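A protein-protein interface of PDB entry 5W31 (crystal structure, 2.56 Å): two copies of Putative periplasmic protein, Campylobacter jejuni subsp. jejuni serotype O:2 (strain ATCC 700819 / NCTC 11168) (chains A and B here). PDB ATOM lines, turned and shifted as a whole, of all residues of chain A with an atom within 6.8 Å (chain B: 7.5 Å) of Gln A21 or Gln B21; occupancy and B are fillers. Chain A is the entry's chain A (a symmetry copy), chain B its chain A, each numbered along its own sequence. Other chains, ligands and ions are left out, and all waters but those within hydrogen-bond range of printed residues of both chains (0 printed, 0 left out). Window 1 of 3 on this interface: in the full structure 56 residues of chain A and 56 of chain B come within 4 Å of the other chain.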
ATOM      1  N   HIS A  19      -6.756 -21.998  15.368  1.00  0.00           N
ATOM      2  CA  HIS A  19      -6.936 -23.342  15.956  1.00  0.00           C
ATOM      3  C   HIS A  19      -6.457 -24.521  15.105  1.00  0.00           C
ATOM      4  O   HIS A  19      -6.392 -24.433  13.872  1.00  0.00           O
ATOM      5  CB  HIS A  19      -8.375 -23.592  16.446  1.00  0.00           C
ATOM      6  CG  HIS A  19      -9.340 -24.006  15.365  1.00  0.00           C
ATOM      7  ND1 HIS A  19      -9.307 -23.480  14.086  1.00  0.00           N
ATOM      8  CD2 HIS A  19     -10.394 -24.863  15.394  1.00  0.00           C
ATOM      9  CE1 HIS A  19     -10.279 -24.019  13.361  1.00  0.00           C
ATOM     10  NE2 HIS A  19     -10.960 -24.851  14.135  1.00  0.00           N
ATOM     11  N   LEU A  20      -6.152 -25.611  15.813  1.00  0.00           N
ATOM     12  CA  LEU A  20      -5.804 -26.897  15.256  1.00  0.00           C
ATOM     13  C   LEU A  20      -7.036 -27.697  14.926  1.00  0.00           C
ATOM     14  O   LEU A  20      -8.034 -27.580  15.612  1.00  0.00           O
ATOM     15  CB  LEU A  20      -4.980 -27.662  16.274  1.00  0.00           C
ATOM     16  CG  LEU A  20      -3.603 -27.055  16.514  1.00  0.00           C
ATOM     17  CD1 LEU A  20      -2.762 -27.968  17.393  1.00  0.00           C
ATOM     18  CD2 LEU A  20      -2.904 -26.769  15.182  1.00  0.00           C
ATOM     19  N   GLN A  21      -6.962 -28.491  13.863  1.00  0.00           N
ATOM     20  CA  GLN A  21      -7.962 -29.518  13.538  1.00  0.00           C
ATOM     21  C   GLN A  21      -7.302 -30.827  13.105  1.00  0.00           C
ATOM     22  O   GLN A  21      -6.445 -30.848  12.220  1.00  0.00           O
ATOM     23  CB  GLN A  21      -8.905 -29.039  12.456  1.00  0.00           C
ATOM     24  CG  GLN A  21      -9.650 -27.772  12.825  1.00  0.00           C
ATOM     25  CD  GLN A  21     -10.772 -27.451  11.857  1.00  0.00           C
ATOM     26  OE1 GLN A  21     -10.530 -27.008  10.729  1.00  0.00           O
ATOM     27  NE2 GLN A  21     -12.016 -27.667  12.297  1.00  0.00           N
ATOM     28  N   ILE A  22      -7.695 -31.910  13.763  1.00  0.00           N
ATOM     29  CA  ILE A  22      -7.299 -33.278  13.411  1.00  0.00           C
ATOM     30  C   ILE A  22      -8.181 -33.741  12.262  1.00  0.00           C
ATOM     31  O   ILE A  22      -9.355 -33.388  12.206  1.00  0.00           O
ATOM     32  CB  ILE A  22      -7.431 -34.208  14.632  1.00  0.00           C
ATOM     33  CG1 ILE A  22      -6.606 -35.495  14.459  1.00  0.00           C
ATOM     34  CG2 ILE A  22      -8.905 -34.452  14.966  1.00  0.00           C
ATOM     35  CD1 ILE A  22      -6.082 -36.113  15.762  1.00  0.00           C
ATOM     36  N   SER A  23      -7.590 -34.455  11.311  1.00  0.00           N
ATOM     37  CA  SER A  23      -8.326 -35.065  10.184  1.00  0.00           C
ATOM     38  C   SER A  23      -7.592 -36.322   9.694  1.00  0.00           C
ATOM     39  O   SER A  23      -6.365 -36.461   9.867  1.00  0.00           O
ATOM     40  CB  SER A  23      -8.569 -34.075   9.033  1.00  0.00           C
ATOM     41  OG  SER A  23      -7.369 -33.826   8.318  1.00  0.00           O
ATOM     42  N   THR A 154       2.464 -33.486  14.225  1.00  0.00           N
ATOM     43  CA  THR A 154       1.826 -33.098  12.945  1.00  0.00           C
ATOM     44  C   THR A 154       1.081 -34.253  12.235  1.00  0.00           C
ATOM     45  O   THR A 154      -0.014 -34.069  11.680  1.00  0.00           O
ATOM     46  CB  THR A 154       2.896 -32.533  11.962  1.00  0.00           C
ATOM     47  OG1 THR A 154       3.706 -31.572  12.645  1.00  0.00           O
ATOM     48  CG2 THR A 154       2.275 -31.918  10.648  1.00  0.00           C
ATOM     49  N   HIS B  19      -3.521 -36.485  10.530  1.00  0.00           N
ATOM     50  CA  HIS B  19      -2.707 -35.274  10.765  1.00  0.00           C
ATOM     51  C   HIS B  19      -3.463 -34.037  11.257  1.00  0.00           C
ATOM     52  O   HIS B  19      -4.667 -33.885  11.012  1.00  0.00           O
ATOM     53  CB  HIS B  19      -1.818 -34.908   9.561  1.00  0.00           C
ATOM     54  CG  HIS B  19      -2.525 -34.144   8.473  1.00  0.00           C
ATOM     55  ND1 HIS B  19      -3.833 -34.401   8.099  1.00  0.00           N
ATOM     56  CD2 HIS B  19      -2.085 -33.157   7.648  1.00  0.00           C
ATOM     57  CE1 HIS B  19      -4.179 -33.586   7.112  1.00  0.00           C
ATOM     58  NE2 HIS B  19      -3.134 -32.830   6.811  1.00  0.00           N
ATOM     59  N   LEU B  20      -2.703 -33.171  11.931  1.00  0.00           N
ATOM     60  CA  LEU B  20      -3.128 -31.868  12.388  1.00  0.00           C
ATOM     61  C   LEU B  20      -2.989 -30.839  11.299  1.00  0.00           C
ATOM     62  O   LEU B  20      -2.088 -30.934  10.487  1.00  0.00           O
ATOM     63  CB  LEU B  20      -2.261 -31.458  13.564  1.00  0.00           C
ATOM     64  CG  LEU B  20      -2.494 -32.305  14.809  1.00  0.00           C
ATOM     65  CD1 LEU B  20      -1.741 -31.727  15.997  1.00  0.00           C
ATOM     66  CD2 LEU B  20      -3.991 -32.424  15.105  1.00  0.00           C
ATOM     67  N   GLN B  21      -3.898 -29.869  11.278  1.00  0.00           N
ATOM     68  CA  GLN B  21      -3.782 -28.657  10.456  1.00  0.00           C
ATOM     69  C   GLN B  21      -4.170 -27.405  11.244  1.00  0.00           C
ATOM     70  O   GLN B  21      -5.236 -27.340  11.857  1.00  0.00           O
ATOM     71  CB  GLN B  21      -4.635 -28.758   9.210  1.00  0.00           C
ATOM     72  CG  GLN B  21      -4.280 -29.944   8.335  1.00  0.00           C
ATOM     73  CD  GLN B  21      -4.951 -29.888   6.976  1.00  0.00           C
ATOM     74  OE1 GLN B  21      -6.157 -30.129   6.854  1.00  0.00           O
ATOM     75  NE2 GLN B  21      -4.167 -29.575   5.939  1.00  0.00           N
ATOM     76  N   ILE B  22      -3.271 -26.428  11.241  1.00  0.00           N
ATOM     77  CA  ILE B  22      -3.501 -25.095  11.809  1.00  0.00           C
ATOM     78  C   ILE B  22      -4.288 -24.282  10.792  1.00  0.00           C
ATOM     79  O   ILE B  22      -4.082 -24.431   9.592  1.00  0.00           O
ATOM     80  CB  ILE B  22      -2.161 -24.418  12.155  1.00  0.00           C
ATOM     81  CG1 ILE B  22      -2.348 -23.266  13.157  1.00  0.00           C
ATOM     82  CG2 ILE B  22      -1.413 -24.022  10.880  1.00  0.00           C
ATOM     83  CD1 ILE B  22      -1.153 -23.010  14.084  1.00  0.00           C
ATOM     84  N   SER B  23      -5.241 -23.491  11.274  1.00  0.00           N
ATOM     85  CA  SER B  23      -6.022 -22.563  10.432  1.00  0.00           C
ATOM     86  C   SER B  23      -6.491 -21.361  11.266  1.00  0.00           C
ATOM     87  O   SER B  23      -6.632 -21.451  12.503  1.00  0.00           O
ATOM     88  CB  SER B  23      -7.205 -23.254   9.733  1.00  0.00           C
ATOM     89  OG  SER B  23      -8.244 -23.536  10.657  1.00  0.00           O
ATOM     90  N   ASN B  24      -6.688 -20.240  10.576  1.00  0.00           N
ATOM     91  CA  ASN B  24      -7.203 -19.013  11.167  1.00  0.00           C
ATOM     92  C   ASN B  24      -8.699 -19.012  11.124  1.00  0.00           C
ATOM     93  O   ASN B  24      -9.264 -19.046  10.021  1.00  0.00           O
ATOM     94  CB  ASN B  24      -6.745 -17.808  10.347  1.00  0.00           C
ATOM     95  CG  ASN B  24      -5.476 -17.189  10.870  1.00  0.00           C
ATOM     96  OD1 ASN B  24      -5.181 -17.233  12.070  1.00  0.00           O
ATOM     97  ND2 ASN B  24      -4.714 -16.590   9.964  1.00  0.00           N
ATOM     98  N   VAL B  25      -9.344 -18.957  12.291  1.00  0.00           N
ATOM     99  CA  VAL B  25     -10.738 -18.487  12.329  1.00  0.00           C
ATOM    100  C   VAL B  25     -10.794 -16.946  12.237  1.00  0.00           C
ATOM    101  O   VAL B  25     -10.261 -16.258  13.133  1.00  0.00           O
ATOM    102  CB  VAL B  25     -11.488 -18.924  13.587  1.00  0.00           C
ATOM    103  CG1 VAL B  25     -12.981 -18.710  13.371  1.00  0.00           C
ATOM    104  CG2 VAL B  25     -11.215 -20.372  13.894  1.00  0.00           C
ATOM    105  N   ARG B  64     -20.964 -22.846  14.793  1.00  0.00           N
ATOM    106  CA  ARG B  64     -19.884 -22.336  15.660  1.00  0.00           C
ATOM    107  C   ARG B  64     -20.319 -21.026  16.320  1.00  0.00           C
ATOM    108  O   ARG B  64     -20.117 -20.832  17.520  1.00  0.00           O
ATOM    109  CB  ARG B  64     -18.572 -22.131  14.903  1.00  0.00           C
ATOM    110  CG  ARG B  64     -17.328 -22.412  15.741  1.00  0.00           C
ATOM    111  CD  ARG B  64     -16.221 -21.429  15.409  1.00  0.00           C
ATOM    112  NE  ARG B  64     -15.483 -21.738  14.179  1.00  0.00           N
ATOM    113  CZ  ARG B  64     -15.745 -21.215  12.976  1.00  0.00           C
ATOM    114  NH1 ARG B  64     -16.750 -20.373  12.798  1.00  0.00           N
ATOM    115  NH2 ARG B  64     -15.015 -21.549  11.930  1.00  0.00           N
ATOM    116  N   ILE B 153      -3.453 -25.324  23.334  1.00  0.00           N
ATOM    117  CA  ILE B 153      -3.051 -26.123  22.188  1.00  0.00           C
ATOM    118  C   ILE B 153      -4.080 -26.111  21.061  1.00  0.00           C
ATOM    119  O   ILE B 153      -3.761 -25.684  19.962  1.00  0.00           O
ATOM    120  CB  ILE B 153      -2.717 -27.548  22.591  1.00  0.00           C
ATOM    121  CG1 ILE B 153      -1.704 -27.529  23.746  1.00  0.00           C
ATOM    122  CG2 ILE B 153      -2.163 -28.276  21.383  1.00  0.00           C
ATOM    123  CD1 ILE B 153      -1.555 -28.834  24.507  1.00  0.00           C
ATOM    124  N   THR B 154      -5.299 -26.560  21.329  1.00  0.00           N
ATOM    125  CA  THR B 154      -6.407 -26.580  20.345  1.00  0.00           C
ATOM    126  C   THR B 154      -6.706 -25.207  19.700  1.00  0.00           C
ATOM    127  O   THR B 154      -6.970 -25.105  18.492  1.00  0.00           O
ATOM    128  CB  THR B 154      -7.714 -27.096  21.020  1.00  0.00           C
ATOM    129  OG1 THR B 154      -7.429 -28.287  21.758  1.00  0.00           O
ATOM    130  CG2 THR B 154      -8.893 -27.332  19.997  1.00  0.00           C
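The backbone NH (N) of His B19 is in hydrogen-bond range of the backbone carbonyl oxygen (O) of Ser A23 (2.9 Å).
The backbone carbonyl oxygen (O) of Thr B154 is in hydrogen-bond range of the backbone NH (N) of Leu A20 (2.8 Å).
N of Leu B20 lies within hydrogen-bond range of O of Thr A154, 2.8 Å away.
The backbone carbonyl oxygen (O) of Gln B21 is in hydrogen-bond range of the backbone NH (N) of Gln A21.
N of His A19 sits at hydrogen-bond distance from O of Ser B23 (2.9 Å).
Hydrophobic or aromatic side chains of chain A within 4 Å of the printed part of chain B: His A19, Leu A20 and Ile A22.
Of the 10 printed residues of chain B, 8 touch a printed residue of chain A.
Printed residues of chain B that touch a printed residue of chain A: His B19, Leu B20, Gln B21, Ile B22, Ser B23, Val B25, Ile B153 and Thr B154.
Hydrophobic or aromatic side chains of chain B within 4 Å of the printed part of chain A: His B19, Leu B20, Ile B22 and Val B25.
Among the printed residues, 17 pairs touch across the chains.
Among the printed residues, merely in contact across the chains: His A19 with Gln B21, His A19 with Ile B22, His A19 with Val B25, His A19 with Thr B154, Leu A20 with Gln B21, Leu A20 with Ile B22, Leu A20 with Ile B153, Gln A21 with His B19, Gln A21 with Leu B20, Ile A22 with His B19, Ile A22 with Leu B20 and Thr A154 with His B19.
Leu A20 touches Gln B21, and with the chains exchanged Gln A21 touches Leu B20.
Leu A20 touches Ile B22, and with the chains exchanged Ile A22 touches Leu B20.
Leu A20 touches Thr B154, and with the chains exchanged Thr A154 touches Leu B20.
Gln A21 touches its own counterpart, Gln B21.
Positions printed for both chains: 19, 20, 21, 22, 23 and 154.
Of the 17 pairs that touch across the chains among the printed residues, 15 have their exchanged pair printed and touching as well.
Gln A21 touches three residues of chain B.
Gln B21 touches just these residues of chain A: His A19 (3.7 Å), Leu A20 (3.5 Å) and Gln A21 (2.9 Å).
Printed residues of chain A within 4 Å of Thr B154: His A19 and Leu A20.
Of the printed residues of chain A, His B19 touches Gln A21 (3.7 Å), Ile A22 (3.6 Å), Ser A23 (2.9 Å) and Thr A154 (2.9 Å).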
